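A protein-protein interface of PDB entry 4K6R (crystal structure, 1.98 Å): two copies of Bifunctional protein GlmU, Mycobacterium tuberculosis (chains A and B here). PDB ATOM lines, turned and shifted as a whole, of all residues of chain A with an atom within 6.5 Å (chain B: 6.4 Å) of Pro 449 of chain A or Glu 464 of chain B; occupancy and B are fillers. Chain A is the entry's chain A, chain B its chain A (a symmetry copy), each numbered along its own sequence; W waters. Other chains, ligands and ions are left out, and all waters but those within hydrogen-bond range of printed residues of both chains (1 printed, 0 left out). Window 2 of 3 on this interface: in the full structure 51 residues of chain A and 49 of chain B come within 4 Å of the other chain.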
ATOM      1  N   THR A 431     -30.106  15.797 -13.297  1.00  0.00           N
ATOM      2  CA  THR A 431     -29.234  16.930 -12.943  1.00  0.00           C
ATOM      3  C   THR A 431     -27.892  16.768 -13.615  1.00  0.00           C
ATOM      4  O   THR A 431     -27.336  15.650 -13.583  1.00  0.00           O
ATOM      5  CB  THR A 431     -28.985  16.968 -11.393  1.00  0.00           C
ATOM      6  OG1 THR A 431     -30.209  17.273 -10.756  1.00  0.00           O
ATOM      7  CG2 THR A 431     -28.029  18.059 -11.003  1.00  0.00           C
ATOM      8  N   ILE A 432     -27.346  17.841 -14.205  1.00  0.00           N
ATOM      9  CA  ILE A 432     -26.028  17.806 -14.811  1.00  0.00           C
ATOM     10  C   ILE A 432     -25.182  18.718 -13.968  1.00  0.00           C
ATOM     11  O   ILE A 432     -25.455  19.933 -13.890  1.00  0.00           O
ATOM     12  CB  ILE A 432     -26.047  18.433 -16.276  1.00  0.00           C
ATOM     13  CG1 ILE A 432     -27.150  17.823 -17.147  1.00  0.00           C
ATOM     14  CG2 ILE A 432     -24.691  18.355 -16.929  1.00  0.00           C
ATOM     15  CD1 ILE A 432     -26.967  16.472 -17.463  1.00  0.00           C
ATOM     16  N   GLY A 433     -24.143  18.192 -13.320  1.00  0.00           N
ATOM     17  CA  GLY A 433     -23.340  19.056 -12.418  1.00  0.00           C
ATOM     18  C   GLY A 433     -22.436  20.048 -13.107  1.00  0.00           C
ATOM     19  O   GLY A 433     -22.227  20.010 -14.331  1.00  0.00           O
ATOM     20  N   ASP A 434     -21.853  20.953 -12.349  1.00  0.00           N
ATOM     21  CA  ASP A 434     -21.026  21.982 -12.924  1.00  0.00           C
ATOM     22  C   ASP A 434     -19.883  21.427 -13.761  1.00  0.00           C
ATOM     23  O   ASP A 434     -19.264  20.452 -13.356  1.00  0.00           O
ATOM     24  CB  ASP A 434     -20.431  22.901 -11.814  1.00  0.00           C
ATOM     25  CG  ASP A 434     -21.497  23.690 -11.031  1.00  0.00           C
ATOM     26  OD1 ASP A 434     -22.694  23.888 -11.461  1.00  0.00           O
ATOM     27  OD2 ASP A 434     -21.111  24.144  -9.935  1.00  0.00           O
ATOM     28  N   GLY A 435     -19.613  22.079 -14.889  1.00  0.00           N
ATOM     29  CA  GLY A 435     -18.469  21.810 -15.749  1.00  0.00           C
ATOM     30  C   GLY A 435     -18.552  20.457 -16.473  1.00  0.00           C
ATOM     31  O   GLY A 435     -17.585  20.080 -17.179  1.00  0.00           O
ATOM     32  N   ALA A 436     -19.676  19.778 -16.402  1.00  0.00           N
ATOM     33  CA  ALA A 436     -19.907  18.563 -17.164  1.00  0.00           C
ATOM     34  C   ALA A 436     -20.026  18.785 -18.671  1.00  0.00           C
ATOM     35  O   ALA A 436     -20.279  19.863 -19.148  1.00  0.00           O
ATOM     36  CB  ALA A 436     -21.099  17.841 -16.664  1.00  0.00           C
ATOM     37  N   TYR A 437     -19.819  17.712 -19.399  1.00  0.00           N
ATOM     38  CA  TYR A 437     -19.950  17.687 -20.828  1.00  0.00           C
ATOM     39  C   TYR A 437     -20.903  16.540 -21.154  1.00  0.00           C
ATOM     40  O   TYR A 437     -21.040  15.643 -20.382  1.00  0.00           O
ATOM     41  CB  TYR A 437     -18.607  17.411 -21.485  1.00  0.00           C
ATOM     42  CG  TYR A 437     -17.733  18.568 -21.916  1.00  0.00           C
ATOM     43  CD1 TYR A 437     -17.332  18.707 -23.219  1.00  0.00           C
ATOM     44  CD2 TYR A 437     -17.258  19.477 -21.011  1.00  0.00           C
ATOM     45  CE1 TYR A 437     -16.527  19.711 -23.605  1.00  0.00           C
ATOM     46  CE2 TYR A 437     -16.454  20.486 -21.399  1.00  0.00           C
ATOM     47  CZ  TYR A 437     -16.092  20.599 -22.697  1.00  0.00           C
ATOM     48  OH  TYR A 437     -15.295  21.593 -23.097  1.00  0.00           O
ATOM     49  N   ASP A 447     -28.280  11.265 -13.673  1.00  0.00           N
ATOM     50  CA  ASP A 447     -27.518  12.404 -13.241  1.00  0.00           C
ATOM     51  C   ASP A 447     -26.129  12.299 -13.753  1.00  0.00           C
ATOM     52  O   ASP A 447     -25.634  11.208 -13.920  1.00  0.00           O
ATOM     53  CB  ASP A 447     -27.495  12.501 -11.686  1.00  0.00           C
ATOM     54  CG  ASP A 447     -28.863  12.901 -11.124  1.00  0.00           C
ATOM     55  OD1 ASP A 447     -29.738  13.305 -11.948  1.00  0.00           O
ATOM     56  OD2 ASP A 447     -29.083  12.781  -9.899  1.00  0.00           O
ATOM     57  N   VAL A 448     -25.490  13.431 -13.984  1.00  0.00           N
ATOM     58  CA  VAL A 448     -24.191  13.452 -14.553  1.00  0.00           C
ATOM     59  C   VAL A 448     -23.355  14.242 -13.527  1.00  0.00           C
ATOM     60  O   VAL A 448     -23.621  15.434 -13.255  1.00  0.00           O
ATOM     61  CB  VAL A 448     -24.178  14.204 -15.888  1.00  0.00           C
ATOM     62  CG1 VAL A 448     -22.724  14.317 -16.391  1.00  0.00           C
ATOM     63  CG2 VAL A 448     -25.051  13.478 -16.942  1.00  0.00           C
ATOM     64  N   PRO A 449     -22.319  13.601 -12.957  1.00  0.00           N
ATOM     65  CA  PRO A 449     -21.474  14.353 -11.946  1.00  0.00           C
ATOM     66  C   PRO A 449     -20.758  15.534 -12.550  1.00  0.00           C
ATOM     67  O   PRO A 449     -20.492  15.536 -13.774  1.00  0.00           O
ATOM     68  CB  PRO A 449     -20.398  13.279 -11.482  1.00  0.00           C
ATOM     69  CG  PRO A 449     -21.096  11.958 -11.716  1.00  0.00           C
ATOM     70  CD  PRO A 449     -21.925  12.178 -13.082  1.00  0.00           C
ATOM     71  N   PRO A 450     -20.370  16.522 -11.704  1.00  0.00           N
ATOM     72  CA  PRO A 450     -19.552  17.633 -12.133  1.00  0.00           C
ATOM     73  C   PRO A 450     -18.294  17.148 -12.854  1.00  0.00           C
ATOM     74  O   PRO A 450     -17.698  16.129 -12.453  1.00  0.00           O
ATOM     75  CB  PRO A 450     -19.185  18.371 -10.779  1.00  0.00           C
ATOM     76  CG  PRO A 450     -20.171  17.968  -9.844  1.00  0.00           C
ATOM     77  CD  PRO A 450     -20.666  16.569 -10.247  1.00  0.00           C
ATOM     78  N   GLY A 451     -17.892  17.815 -13.932  1.00  0.00           N
ATOM     79  CA  GLY A 451     -16.639  17.402 -14.594  1.00  0.00           C
ATOM     80  C   GLY A 451     -16.650  16.034 -15.291  1.00  0.00           C
ATOM     81  O   GLY A 451     -15.640  15.642 -15.887  1.00  0.00           O
ATOM     82  N   ALA A 452     -17.779  15.319 -15.229  1.00  0.00           N
ATOM     83  CA  ALA A 452     -17.959  14.058 -16.024  1.00  0.00           C
ATOM     84  C   ALA A 452     -18.307  14.316 -17.535  1.00  0.00           C
ATOM     85  O   ALA A 452     -18.815  15.433 -17.900  1.00  0.00           O
ATOM     86  CB  ALA A 452     -19.036  13.184 -15.330  1.00  0.00           C
ATOM     87  N   LEU A 453     -17.955  13.377 -18.429  1.00  0.00           N
ATOM     88  CA  LEU A 453     -18.468  13.403 -19.805  1.00  0.00           C
ATOM     89  C   LEU A 453     -19.557  12.306 -19.872  1.00  0.00           C
ATOM     90  O   LEU A 453     -19.241  11.132 -19.650  1.00  0.00           O
ATOM     91  CB  LEU A 453     -17.343  13.119 -20.838  1.00  0.00           C
ATOM     92  CG  LEU A 453     -17.772  12.801 -22.307  1.00  0.00           C
ATOM     93  CD1 LEU A 453     -18.492  13.956 -23.011  1.00  0.00           C
ATOM     94  CD2 LEU A 453     -16.587  12.446 -23.201  1.00  0.00           C
ATOM     95  N   ASN B 462     -21.353   7.522 -17.968  1.00  0.00           N
ATOM     96  CA  ASN B 462     -20.656   8.682 -17.461  1.00  0.00           C
ATOM     97  C   ASN B 462     -19.170   8.426 -17.320  1.00  0.00           C
ATOM     98  O   ASN B 462     -18.799   7.511 -16.615  1.00  0.00           O
ATOM     99  CB  ASN B 462     -21.169   9.076 -16.081  1.00  0.00           C
ATOM    100  CG  ASN B 462     -22.583   9.651 -16.127  1.00  0.00           C
ATOM    101  OD1 ASN B 462     -23.031  10.140 -17.166  1.00  0.00           O
ATOM    102  ND2 ASN B 462     -23.267   9.626 -14.989  1.00  0.00           N
ATOM    103  N   ILE B 463     -18.352   9.240 -17.973  1.00  0.00           N
ATOM    104  CA  ILE B 463     -16.882   9.111 -17.919  1.00  0.00           C
ATOM    105  C   ILE B 463     -16.435  10.180 -16.897  1.00  0.00           C
ATOM    106  O   ILE B 463     -16.360  11.377 -17.236  1.00  0.00           O
ATOM    107  CB  ILE B 463     -16.267   9.350 -19.288  1.00  0.00           C
ATOM    108  CG1 ILE B 463     -16.892   8.396 -20.315  1.00  0.00           C
ATOM    109  CG2 ILE B 463     -14.720   9.151 -19.259  1.00  0.00           C
ATOM    110  CD1 ILE B 463     -16.559   8.771 -21.724  1.00  0.00           C
ATOM    111  N   GLU B 464     -16.176   9.745 -15.655  1.00  0.00           N
ATOM    112  CA  GLU B 464     -15.886  10.677 -14.588  1.00  0.00           C
ATOM    113  C   GLU B 464     -14.508  11.352 -14.732  1.00  0.00           C
ATOM    114  O   GLU B 464     -13.550  10.727 -15.213  1.00  0.00           O
ATOM    115  CB  GLU B 464     -16.053   9.987 -13.269  1.00  0.00           C
ATOM    116  CG  GLU B 464     -17.516   9.728 -12.942  1.00  0.00           C
ATOM    117  CD  GLU B 464     -17.660   9.149 -11.546  1.00  0.00           C
ATOM    118  OE1 GLU B 464     -17.238   8.002 -11.380  1.00  0.00           O
ATOM    119  OE2 GLU B 464     -18.118   9.854 -10.611  1.00  0.00           O
ATOM    120  N   ASN B 465     -14.455  12.656 -14.419  1.00  0.00           N
ATOM    121  CA  ASN B 465     -13.241  13.464 -14.451  1.00  0.00           C
ATOM    122  C   ASN B 465     -12.681  13.606 -15.847  1.00  0.00           C
ATOM    123  O   ASN B 465     -11.518  14.047 -16.021  1.00  0.00           O
ATOM    124  CB  ASN B 465     -12.158  12.936 -13.468  1.00  0.00           C
ATOM    125  CG  ASN B 465     -12.697  12.790 -12.043  1.00  0.00           C
ATOM    126  OD1 ASN B 465     -13.127  13.770 -11.426  1.00  0.00           O
ATOM    127  ND2 ASN B 465     -12.772  11.549 -11.558  1.00  0.00           N
ATOM    128  N   TRP B 466     -13.492  13.264 -16.852  1.00  0.00           N
ATOM    129  CA  TRP B 466     -13.114  13.536 -18.256  1.00  0.00           C
ATOM    130  C   TRP B 466     -12.600  14.982 -18.469  1.00  0.00           C
ATOM    131  O   TRP B 466     -11.578  15.222 -19.145  1.00  0.00           O
ATOM    132  CB  TRP B 466     -14.256  13.221 -19.225  1.00  0.00           C
ATOM    133  CG  TRP B 466     -13.812  13.311 -20.672  1.00  0.00           C
ATOM    134  CD1 TRP B 466     -13.209  12.331 -21.412  1.00  0.00           C
ATOM    135  CD2 TRP B 466     -13.908  14.456 -21.522  1.00  0.00           C
ATOM    136  NE1 TRP B 466     -12.928  12.794 -22.692  1.00  0.00           N
ATOM    137  CE2 TRP B 466     -13.358  14.095 -22.783  1.00  0.00           C
ATOM    138  CE3 TRP B 466     -14.421  15.750 -21.350  1.00  0.00           C
ATOM    139  CZ2 TRP B 466     -13.298  14.995 -23.858  1.00  0.00           C
ATOM    140  CZ3 TRP B 466     -14.363  16.650 -22.428  1.00  0.00           C
ATOM    141  CH2 TRP B 466     -13.801  16.274 -23.648  1.00  0.00           C
ATOM    142  N   VAL B 467     -13.294  15.945 -17.867  1.00  0.00           N
ATOM    143  CA  VAL B 467     -13.059  17.346 -18.212  1.00  0.00           C
ATOM    144  C   VAL B 467     -11.711  17.849 -17.625  1.00  0.00           C
ATOM    145  O   VAL B 467     -10.978  18.522 -18.341  1.00  0.00           O
ATOM    146  CB  VAL B 467     -14.282  18.277 -17.781  1.00  0.00           C
ATOM    147  CG1 VAL B 467     -13.990  19.791 -18.027  1.00  0.00           C
ATOM    148  CG2 VAL B 467     -15.587  17.850 -18.552  1.00  0.00           C
ATOM    149  N   ARG B 469      -9.187  16.023 -17.302  1.00  0.00           N
ATOM    150  CA  ARG B 469      -8.178  15.342 -18.108  1.00  0.00           C
ATOM    151  C   ARG B 469      -8.040  15.923 -19.493  1.00  0.00           C
ATOM    152  O   ARG B 469      -6.916  16.089 -19.984  1.00  0.00           O
ATOM    153  CB  ARG B 469      -8.448  13.820 -18.208  1.00  0.00           C
ATOM    154  CG  ARG B 469      -8.285  13.066 -16.848  1.00  0.00           C
ATOM    155  CD  ARG B 469      -8.089  11.574 -17.149  1.00  0.00           C
ATOM    156  NE  ARG B 469      -9.249  11.006 -17.860  1.00  0.00           N
ATOM    157  CZ  ARG B 469     -10.316  10.532 -17.222  1.00  0.00           C
ATOM    158  NH1 ARG B 469     -10.319  10.559 -15.893  1.00  0.00           N
ATOM    159  NH2 ARG B 469     -11.356  10.005 -17.895  1.00  0.00           N
HETATM  160  O   HOH W   1     -16.658  13.556 -12.929  1.00  0.00           O
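Water W1 lies within hydrogen-bond range of N of Asn 465 of chain B (2.8 Å), O of Pro 450 of chain A (2.8 Å) and N of Ala 452 of chain A (3.1 Å).
No position is printed for both chains. Of the 14 pairs that touch across the chains among the printed residues, none has its exchanged pair printed and touching as well.
Among the printed residues, pairs that only touch across the chains: Gly 435 of chain A with Val 467 of chain B, Tyr 437 of chain A with Trp 466 of chain B, Tyr 437 of chain A with Val 467 of chain B, Val 448 of chain A with Asn 462 of chain B, Pro 449 of chain A with Asn 462 of chain B, Pro 449 of chain A with Glu 464 of chain B, Gly 451 of chain A with Asn 465 of chain B, Ala 452 of chain A with Ile 463 of chain B, Leu 453 of chain A with Asn 462 of chain B and Leu 453 of chain A with Trp 466 of chain B.
The side-chain carboxylate of Asp 447 of chain A sits at hydrogen-bond distance from the backbone NH of Thr 431 of chain A, 2.9 Å away. O of Thr 431 of chain A sits at hydrogen-bond distance from N of Val 448 of chain A. The backbone carbonyl oxygen (O) of Val 448 of chain A sits at hydrogen-bond distance from the backbone NH (N) of Gly 433 of chain A, at 2.8 Å. The backbone NH (N) of Gly 451 of chain A is in hydrogen-bond range of the backbone carbonyl oxygen (O) of Asp 434 of chain A (3.0 Å). O of Ala 452 of chain A is in hydrogen-bond range of N of Tyr 437 of chain A (2.9 Å). The backbone carbonyl oxygen of Glu 464 of chain B lies within hydrogen-bond range of the guanidinium group of Arg 469 of chain B (3.3 Å).
Pro 449 of chain A touches just these residues of chain B: Asn 462 (3.5 Å) and Glu 464 (3.8 Å). Glu 464 of chain B touches one residue of chain A. Of the printed residues of chain A, Ile 463 of chain B touches Ala 452 and Leu 453. Of the printed residues of chain B, Gly 435 of chain A touches Val 467 (3.3 Å). Of the printed residues of chain B, Leu 453 of chain A touches Asn 462 (3.6 Å), Ile 463 (2.7 Å) and Trp 466 (3.5 Å). Ala 436 of chain A touches none of the printed residues of chain B. The nearest printed residue of chain B that does not touch Pro 449 of chain A is Asn 465 of chain B (6.7 Å).
The side-chain amide nitrogen (ND2) of Asn 462 of chain B lies within hydrogen-bond range of the backbone carbonyl oxygen (O) of Asp 447 of chain A (3.0 Å). The backbone NH (N) of Trp 466 of chain B is in hydrogen-bond range of the backbone carbonyl oxygen (O) of Gly 451 of chain A (3.3 Å). The backbone NH (N) of Val 467 of chain B sits at hydrogen-bond distance from the backbone carbonyl oxygen (O) of Gly 451 of chain A, at 3.1 Å. N of Ile 463 of chain B lies within hydrogen-bond range of O of Leu 453 of chain A, at 2.7 Å.
Hydrophobic or aromatic side chains of chain B that line the printed part of chain A: Ile 463, Trp 466 and Val 467. Printed residues of chain A that touch a printed residue of chain B: Gly 435, Tyr 437, Asp 447, Val 448, Pro 449, Gly 451, Ala 452 and Leu 453. Hydrophobic or aromatic side chains of chain A within 4 Å of the printed part of chain B: Tyr 437, Val 448, Pro 449, Ala 452 and Leu 453. Along chain A the printed residues that touch a printed residue of chain B span positions 435 to 453. Among the printed residues, 14 pairs touch across the chains. Among the printed residues, no Asp or Glu carboxylate lies within 4 Å of a Lys or Arg side-chain nitrogen of the other chain.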
